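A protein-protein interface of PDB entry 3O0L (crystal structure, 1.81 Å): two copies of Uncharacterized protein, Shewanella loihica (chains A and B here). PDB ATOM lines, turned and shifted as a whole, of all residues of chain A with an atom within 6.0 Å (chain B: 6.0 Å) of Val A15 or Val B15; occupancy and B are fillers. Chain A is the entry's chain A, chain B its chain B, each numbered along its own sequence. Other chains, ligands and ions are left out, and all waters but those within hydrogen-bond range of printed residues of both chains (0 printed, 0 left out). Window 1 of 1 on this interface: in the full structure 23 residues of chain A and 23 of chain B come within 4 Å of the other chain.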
ATOM      1  N   ILE A   7      14.687  20.429 -20.058  1.00  0.00           N
ATOM      2  CA  ILE A   7      14.282  19.094 -20.311  1.00  0.00           C
ATOM      3  C   ILE A   7      14.407  18.287 -19.026  1.00  0.00           C
ATOM      4  O   ILE A   7      15.414  18.416 -18.304  1.00  0.00           O
ATOM      5  CB  ILE A   7      15.250  18.464 -21.332  1.00  0.00           C
ATOM      6  CG1 ILE A   7      15.035  19.104 -22.705  1.00  0.00           C
ATOM      7  CG2 ILE A   7      15.094  16.945 -21.390  1.00  0.00           C
ATOM      8  CD1 ILE A   7      15.908  18.488 -23.786  1.00  0.00           C
ATOM      9  N   MET A   8      13.449  17.428 -18.747  1.00  0.00           N
ATOM     10  CA  MET A   8      13.599  16.482 -17.640  1.00  0.00           C
ATOM     11  C   MET A   8      13.211  15.097 -18.130  1.00  0.00           C
ATOM     12  O   MET A   8      12.169  14.917 -18.772  1.00  0.00           O
ATOM     13  CB  MET A   8      12.757  16.912 -16.406  1.00  0.00           C
ATOM     14  CG  MET A   8      12.781  15.897 -15.271  1.00  0.00           C
ATOM     15  SD  MET A   8      12.043  16.645 -13.657  1.00  0.00           S
ATOM     16  CE  MET A   8      10.244  16.429 -13.953  1.00  0.00           C
ATOM     17  N   ILE A   9      14.040  14.133 -17.779  1.00  0.00           N
ATOM     18  CA  ILE A   9      13.887  12.729 -18.128  1.00  0.00           C
ATOM     19  C   ILE A   9      13.720  11.919 -16.882  1.00  0.00           C
ATOM     20  O   ILE A   9      14.455  12.113 -15.901  1.00  0.00           O
ATOM     21  CB  ILE A   9      15.181  12.214 -18.841  1.00  0.00           C
ATOM     22  CG1 ILE A   9      15.517  13.110 -20.034  1.00  0.00           C
ATOM     23  CG2 ILE A   9      15.043  10.745 -19.248  1.00  0.00           C
ATOM     24  CD1 ILE A   9      17.055  13.179 -20.270  1.00  0.00           C
ATOM     25  N   SER A  10      12.806  10.959 -16.897  1.00  0.00           N
ATOM     26  CA  SER A  10      12.654  10.021 -15.780  1.00  0.00           C
ATOM     27  C   SER A  10      13.151   8.626 -16.192  1.00  0.00           C
ATOM     28  O   SER A  10      13.175   8.289 -17.363  1.00  0.00           O
ATOM     29  CB  SER A  10      11.196   9.878 -15.378  1.00  0.00           C
ATOM     30  OG  SER A  10      10.542   9.041 -16.345  1.00  0.00           O
ATOM     31  N   GLY A  13      10.815   6.485 -18.468  1.00  0.00           N
ATOM     32  CA  GLY A  13      10.579   6.813 -19.863  1.00  0.00           C
ATOM     33  C   GLY A  13       9.816   8.089 -20.172  1.00  0.00           C
ATOM     34  O   GLY A  13       9.401   8.325 -21.311  1.00  0.00           O
ATOM     35  N   GLU A  14       9.551   8.881 -19.153  1.00  0.00           N
ATOM     36  CA  GLU A  14       8.862  10.105 -19.358  1.00  0.00           C
ATOM     37  C   GLU A  14       9.844  11.220 -19.654  1.00  0.00           C
ATOM     38  O   GLU A  14      10.858  11.368 -18.940  1.00  0.00           O
ATOM     39  CB  GLU A  14       8.022  10.444 -18.129  1.00  0.00           C
ATOM     40  CG  GLU A  14       7.071  11.615 -18.377  1.00  0.00           C
ATOM     41  CD  GLU A  14       5.963  11.806 -17.323  1.00  0.00           C
ATOM     42  OE1 GLU A  14       5.697  10.909 -16.500  1.00  0.00           O
ATOM     43  OE2 GLU A  14       5.332  12.883 -17.355  1.00  0.00           O
ATOM     44  N   VAL A  15       9.538  12.042 -20.659  1.00  0.00           N
ATOM     45  CA  VAL A  15      10.404  13.151 -21.061  1.00  0.00           C
ATOM     46  C   VAL A  15       9.547  14.371 -21.248  1.00  0.00           C
ATOM     47  O   VAL A  15       8.549  14.342 -21.997  1.00  0.00           O
ATOM     48  CB  VAL A  15      11.183  12.904 -22.362  1.00  0.00           C
ATOM     49  CG1 VAL A  15      12.050  14.119 -22.707  1.00  0.00           C
ATOM     50  CG2 VAL A  15      12.076  11.652 -22.223  1.00  0.00           C
ATOM     51  N   ARG A  16       9.905  15.428 -20.539  1.00  0.00           N
ATOM     52  CA  ARG A  16       9.244  16.689 -20.718  1.00  0.00           C
ATOM     53  C   ARG A  16      10.217  17.768 -21.127  1.00  0.00           C
ATOM     54  O   ARG A  16      11.366  17.791 -20.690  1.00  0.00           O
ATOM     55  CB  ARG A  16       8.437  17.084 -19.505  1.00  0.00           C
ATOM     56  CG  ARG A  16       9.169  17.382 -18.304  1.00  0.00           C
ATOM     57  CD  ARG A  16       8.178  17.875 -17.161  1.00  0.00           C
ATOM     58  NE  ARG A  16       7.681  19.217 -17.419  1.00  0.00           N
ATOM     59  CZ  ARG A  16       6.541  19.724 -16.931  1.00  0.00           C
ATOM     60  NH1 ARG A  16       5.756  19.010 -16.130  1.00  0.00           N
ATOM     61  NH2 ARG A  16       6.182  20.960 -17.248  1.00  0.00           N
ATOM     62  N   VAL A  17       9.709  18.649 -21.974  1.00  0.00           N
ATOM     63  CA  VAL A  17      10.426  19.778 -22.540  1.00  0.00           C
ATOM     64  C   VAL A  17       9.612  21.029 -22.255  1.00  0.00           C
ATOM     65  O   VAL A  17       8.375  21.070 -22.499  1.00  0.00           O
ATOM     66  CB  VAL A  17      10.598  19.606 -24.073  1.00  0.00           C
ATOM     67  CG1 VAL A  17      11.286  20.844 -24.700  1.00  0.00           C
ATOM     68  CG2 VAL A  17      11.338  18.312 -24.382  1.00  0.00           C
ATOM     69  N   SER A  24       6.014  20.090 -23.918  1.00  0.00           N
ATOM     70  CA  SER A  24       5.579  18.753 -24.222  1.00  0.00           C
ATOM     71  C   SER A  24       5.914  17.834 -23.080  1.00  0.00           C
ATOM     72  O   SER A  24       6.762  18.134 -22.278  1.00  0.00           O
ATOM     73  CB  SER A  24       6.257  18.238 -25.480  1.00  0.00           C
ATOM     74  OG  SER A  24       7.641  18.269 -25.318  1.00  0.00           O
ATOM     75  N   ASP A  25       5.226  16.710 -23.015  1.00  0.00           N
ATOM     76  CA  ASP A  25       5.399  15.759 -21.956  1.00  0.00           C
ATOM     77  C   ASP A  25       4.931  14.445 -22.508  1.00  0.00           C
ATOM     78  O   ASP A  25       3.733  14.257 -22.708  1.00  0.00           O
ATOM     79  CB  ASP A  25       4.570  16.206 -20.746  1.00  0.00           C
ATOM     80  CG  ASP A  25       4.882  15.429 -19.474  1.00  0.00           C
ATOM     81  OD1 ASP A  25       5.469  14.342 -19.539  1.00  0.00           O
ATOM     82  OD2 ASP A  25       4.509  15.936 -18.391  1.00  0.00           O
ATOM     83  N   VAL A  26       5.871  13.564 -22.800  1.00  0.00           N
ATOM     84  CA  VAL A  26       5.535  12.289 -23.414  1.00  0.00           C
ATOM     85  C   VAL A  26       6.208  11.145 -22.702  1.00  0.00           C
ATOM     86  O   VAL A  26       7.299  11.297 -22.129  1.00  0.00           O
ATOM     87  CB  VAL A  26       5.938  12.252 -24.872  1.00  0.00           C
ATOM     88  CG1 VAL A  26       5.394  13.484 -25.594  1.00  0.00           C
ATOM     89  CG2 VAL A  26       7.448  12.126 -24.999  1.00  0.00           C
ATOM     90  N   ASP A  27       5.523  10.008 -22.690  1.00  0.00           N
ATOM     91  CA  ASP A  27       6.040   8.790 -22.147  1.00  0.00           C
ATOM     92  C   ASP A  27       6.121   7.715 -23.235  1.00  0.00           C
ATOM     93  O   ASP A  27       5.140   7.463 -23.919  1.00  0.00           O
ATOM     94  CB  ASP A  27       5.157   8.312 -21.020  1.00  0.00           C
ATOM     95  CG  ASP A  27       5.750   7.105 -20.324  1.00  0.00           C
ATOM     96  OD1 ASP A  27       6.851   7.234 -19.761  1.00  0.00           O
ATOM     97  OD2 ASP A  27       5.156   6.014 -20.385  1.00  0.00           O
ATOM     98  N   GLU A 108      10.464  14.304 -31.876  1.00  0.00           N
ATOM     99  CA  GLU A 108       9.580  15.452 -31.886  1.00  0.00           C
ATOM    100  C   GLU A 108      10.416  16.685 -32.103  1.00  0.00           C
ATOM    101  O   GLU A 108      11.600  16.719 -31.753  1.00  0.00           O
ATOM    102  CB  GLU A 108       8.787  15.567 -30.574  1.00  0.00           C
ATOM    103  CG  GLU A 108       9.667  15.567 -29.344  1.00  0.00           C
ATOM    104  CD  GLU A 108       8.924  15.929 -28.051  1.00  0.00           C
ATOM    105  OE1 GLU A 108       8.723  17.153 -27.794  1.00  0.00           O
ATOM    106  OE2 GLU A 108       8.571  14.988 -27.291  1.00  0.00           O
ATOM    107  N   ILE B   7      14.268  16.538 -30.640  1.00  0.00           N
ATOM    108  CA  ILE B   7      14.592  15.577 -29.601  1.00  0.00           C
ATOM    109  C   ILE B   7      14.141  14.181 -30.040  1.00  0.00           C
ATOM    110  O   ILE B   7      13.114  14.012 -30.726  1.00  0.00           O
ATOM    111  CB  ILE B   7      13.981  15.978 -28.218  1.00  0.00           C
ATOM    112  CG1 ILE B   7      14.475  15.091 -27.082  1.00  0.00           C
ATOM    113  CG2 ILE B   7      12.483  15.902 -28.254  1.00  0.00           C
ATOM    114  CD1 ILE B   7      13.846  15.456 -25.733  1.00  0.00           C
ATOM    115  N   MET B   8      14.945  13.199 -29.649  1.00  0.00           N
ATOM    116  CA  MET B   8      14.647  11.802 -29.884  1.00  0.00           C
ATOM    117  C   MET B   8      14.719  11.057 -28.565  1.00  0.00           C
ATOM    118  O   MET B   8      15.645  11.237 -27.769  1.00  0.00           O
ATOM    119  CB  MET B   8      15.623  11.179 -30.891  1.00  0.00           C
ATOM    120  CG  MET B   8      15.219   9.779 -31.249  1.00  0.00           C
ATOM    121  SD  MET B   8      16.313   9.007 -32.613  1.00  0.00           S
ATOM    122  CE  MET B   8      17.923   8.766 -31.631  1.00  0.00           C
ATOM    123  N   ILE B   9      13.713  10.239 -28.319  1.00  0.00           N
ATOM    124  CA  ILE B   9      13.568   9.499 -27.095  1.00  0.00           C
ATOM    125  C   ILE B   9      13.437   8.041 -27.490  1.00  0.00           C
ATOM    126  O   ILE B   9      12.749   7.731 -28.483  1.00  0.00           O
ATOM    127  CB  ILE B   9      12.251   9.895 -26.422  1.00  0.00           C
ATOM    128  CG1 ILE B   9      12.254  11.364 -26.092  1.00  0.00           C
ATOM    129  CG2 ILE B   9      11.989   9.097 -25.158  1.00  0.00           C
ATOM    130  CD1 ILE B   9      10.809  11.849 -25.918  1.00  0.00           C
ATOM    131  N   SER B  10      14.062   7.146 -26.721  1.00  0.00           N
ATOM    132  CA  SER B  10      13.969   5.708 -26.981  1.00  0.00           C
ATOM    133  C   SER B  10      13.431   4.963 -25.770  1.00  0.00           C
ATOM    134  O   SER B  10      13.596   5.413 -24.637  1.00  0.00           O
ATOM    135  CB  SER B  10      15.347   5.171 -27.359  1.00  0.00           C
ATOM    136  OG  SER B  10      15.354   3.767 -27.484  1.00  0.00           O
ATOM    137  N   GLY B  13      15.794   4.240 -22.911  1.00  0.00           N
ATOM    138  CA  GLY B  13      16.144   5.363 -22.024  1.00  0.00           C
ATOM    139  C   GLY B  13      17.039   6.421 -22.636  1.00  0.00           C
ATOM    140  O   GLY B  13      17.432   7.366 -21.951  1.00  0.00           O
ATOM    141  N   GLU B  14      17.350   6.313 -23.923  1.00  0.00           N
ATOM    142  CA  GLU B  14      18.139   7.340 -24.576  1.00  0.00           C
ATOM    143  C   GLU B  14      17.329   8.590 -24.782  1.00  0.00           C
ATOM    144  O   GLU B  14      16.159   8.524 -25.187  1.00  0.00           O
ATOM    145  CB  GLU B  14      18.664   6.862 -25.942  1.00  0.00           C
ATOM    146  CG  GLU B  14      19.720   7.872 -26.519  1.00  0.00           C
ATOM    147  CD  GLU B  14      20.228   7.540 -27.903  1.00  0.00           C
ATOM    148  OE1 GLU B  14      19.765   6.538 -28.507  1.00  0.00           O
ATOM    149  OE2 GLU B  14      21.093   8.303 -28.398  1.00  0.00           O
ATOM    150  N   VAL B  15      17.935   9.748 -24.527  1.00  0.00           N
ATOM    151  CA  VAL B  15      17.348  11.028 -24.951  1.00  0.00           C
ATOM    152  C   VAL B  15      18.415  11.838 -25.661  1.00  0.00           C
ATOM    153  O   VAL B  15      19.512  12.108 -25.090  1.00  0.00           O
ATOM    154  CB  VAL B  15      16.791  11.823 -23.771  1.00  0.00           C
ATOM    155  CG1 VAL B  15      16.155  13.158 -24.276  1.00  0.00           C
ATOM    156  CG2 VAL B  15      15.797  10.965 -23.031  1.00  0.00           C
ATOM    157  N   ARG B  16      18.132  12.213 -26.905  1.00  0.00           N
ATOM    158  CA  ARG B  16      19.094  12.989 -27.700  1.00  0.00           C
ATOM    159  C   ARG B  16      18.461  14.297 -28.117  1.00  0.00           C
ATOM    160  O   ARG B  16      17.345  14.314 -28.649  1.00  0.00           O
ATOM    161  CB  ARG B  16      19.542  12.204 -28.935  1.00  0.00           C
ATOM    162  CG  ARG B  16      20.628  12.910 -29.768  1.00  0.00           C
ATOM    163  CD  ARG B  16      20.990  12.096 -31.028  1.00  0.00           C
ATOM    164  NE  ARG B  16      21.745  12.871 -32.001  1.00  0.00           N
ATOM    165  CZ  ARG B  16      23.070  12.997 -31.991  1.00  0.00           C
ATOM    166  NH1 ARG B  16      23.796  12.420 -31.041  1.00  0.00           N
ATOM    167  NH2 ARG B  16      23.673  13.725 -32.919  1.00  0.00           N
ATOM    168  N   VAL B  17      19.181  15.399 -27.884  1.00  0.00           N
ATOM    169  CA  VAL B  17      18.721  16.710 -28.257  1.00  0.00           C
ATOM    170  C   VAL B  17      19.736  17.344 -29.216  1.00  0.00           C
ATOM    171  O   VAL B  17      20.921  17.268 -29.016  1.00  0.00           O
ATOM    172  CB  VAL B  17      18.540  17.648 -27.045  1.00  0.00           C
ATOM    173  CG1 VAL B  17      17.933  18.993 -27.489  1.00  0.00           C
ATOM    174  CG2 VAL B  17      17.682  17.024 -26.014  1.00  0.00           C
ATOM    175  N   SER B  24      23.049  17.239 -27.012  1.00  0.00           N
ATOM    176  CA  SER B  24      23.216  16.360 -25.865  1.00  0.00           C
ATOM    177  C   SER B  24      22.725  14.989 -26.215  1.00  0.00           C
ATOM    178  O   SER B  24      21.867  14.823 -27.092  1.00  0.00           O
ATOM    179  CB  SER B  24      22.489  16.855 -24.604  1.00  0.00           C
ATOM    180  OG  SER B  24      21.077  16.818 -24.743  1.00  0.00           O
ATOM    181  N   ASP B  25      23.246  14.002 -25.502  1.00  0.00           N
ATOM    182  CA  ASP B  25      22.831  12.635 -25.756  1.00  0.00           C
ATOM    183  C   ASP B  25      23.224  11.783 -24.554  1.00  0.00           C
ATOM    184  O   ASP B  25      24.395  11.646 -24.225  1.00  0.00           O
ATOM    185  CB  ASP B  25      23.501  12.138 -27.050  1.00  0.00           C
ATOM    186  CG  ASP B  25      22.783  10.957 -27.686  1.00  0.00           C
ATOM    187  OD1 ASP B  25      21.917  10.318 -27.046  1.00  0.00           O
ATOM    188  OD2 ASP B  25      23.103  10.681 -28.866  1.00  0.00           O
ATOM    189  N   VAL B  26      22.225  11.230 -23.881  1.00  0.00           N
ATOM    190  CA  VAL B  26      22.444  10.421 -22.710  1.00  0.00           C
ATOM    191  C   VAL B  26      21.435   9.298 -22.669  1.00  0.00           C
ATOM    192  O   VAL B  26      20.424   9.322 -23.373  1.00  0.00           O
ATOM    193  CB  VAL B  26      22.352  11.255 -21.384  1.00  0.00           C
ATOM    194  CG1 VAL B  26      23.325  12.401 -21.411  1.00  0.00           C
ATOM    195  CG2 VAL B  26      20.904  11.798 -21.196  1.00  0.00           C
ATOM    196  N   ASP B  27      21.740   8.275 -21.886  1.00  0.00           N
ATOM    197  CA  ASP B  27      20.788   7.198 -21.615  1.00  0.00           C
ATOM    198  C   ASP B  27      20.623   7.072 -20.099  1.00  0.00           C
ATOM    199  O   ASP B  27      21.616   6.991 -19.396  1.00  0.00           O
ATOM    200  CB  ASP B  27      21.330   5.898 -22.193  1.00  0.00           C
ATOM    201  CG  ASP B  27      20.325   4.776 -22.181  1.00  0.00           C
ATOM    202  OD1 ASP B  27      20.078   4.181 -21.104  1.00  0.00           O
ATOM    203  OD2 ASP B  27      19.823   4.442 -23.274  1.00  0.00           O
ATOM    204  N   VAL B  28      19.371   7.041 -19.622  1.00  0.00           N
ATOM    205  CA  VAL B  28      19.047   6.886 -18.215  1.00  0.00           C
ATOM    206  C   VAL B  28      18.383   5.511 -18.046  1.00  0.00           C
ATOM    207  O   VAL B  28      17.406   5.197 -18.731  1.00  0.00           O
ATOM    208  CB  VAL B  28      18.109   7.992 -17.728  1.00  0.00           C
ATOM    209  CG1 VAL B  28      17.878   7.853 -16.211  1.00  0.00           C
ATOM    210  CG2 VAL B  28      18.674   9.388 -18.087  1.00  0.00           C
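The backbone NH of Ile B7 is in hydrogen-bond range of the backbone carbonyl oxygen of Glu A108, 2.9 Å away.
N of Val A15 is in hydrogen-bond range of O of Val A26 (2.8 Å). The side-chain hydroxyl (OG) of Ser A24 is in hydrogen-bond range of the side-chain carboxylate (OE1) of Glu A108 (2.9 Å). O of Val B26 sits at hydrogen-bond distance from N of Val B15, 2.8 Å away. O of Ser B24 sits at hydrogen-bond distance from N of Val B17 (2.9 Å).
Among the printed residues, pairs that only touch across the chains: Ile A7 with Val B17, Ile A9 with Val B15, Val A15 with Ile B7, Val A15 with Ile B9, Val A15 with Val B15 and Val A26 with Ile B9.
Of the printed residues of chain B, Ile A7 touches Val B17 (3.2 Å). Of the printed residues of chain B, Ile A9 touches Val B15. Printed residues of chain B within 4 Å of Val A15: Ile B7 (3.8 Å), Ile B9 (3.7 Å) and Val B15 (3.9 Å). Asp A25 touches none of the printed residues of chain B. Printed residues of chain B within 4 Å of Val A26: Ile B9. Of the printed residues of chain A, Ile B9 touches Val A15 (3.7 Å) and Val A26 (3.5 Å). Printed residues of chain A within 4 Å of Val B15: Ile A9 (3.7 Å) and Val A15 (3.9 Å). Of the printed residues of chain A, Val B17 touches Ile A7. Ser B24 touches none of the printed residues of chain A. The nearest printed residue of chain B that does not touch Val A15 is Glu B14 (5.9 Å).
Of the 14 printed residues of chain A, 5 touch a printed residue of chain B. Along chain A the printed residues that touch a printed residue of chain B span positions 7 to 108. Printed residues of chain B that touch a printed residue of chain A: Ile B7, Ile B9, Val B15 and Val B17. Hydrophobic or aromatic side chains of chain B that line the printed part of chain A: Ile B7, Ile B9, Val B15 and Val B17. Among the printed residues, 7 pairs touch across the chains.
Ile A7 touches Val B17, but with the chains exchanged Val A17 does not touch Ile B7 (4.03 Å). Ile A9 touches Val B15, and with the chains exchanged Val A15 touches Ile B9. Val A15 touches Ile B7, but with the chains exchanged Ile A7 does not touch Val B15 (4.9 Å). Val A26 touches Ile B9, but with the chains exchanged Ile A9 does not touch Val B26 (4.2 Å).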
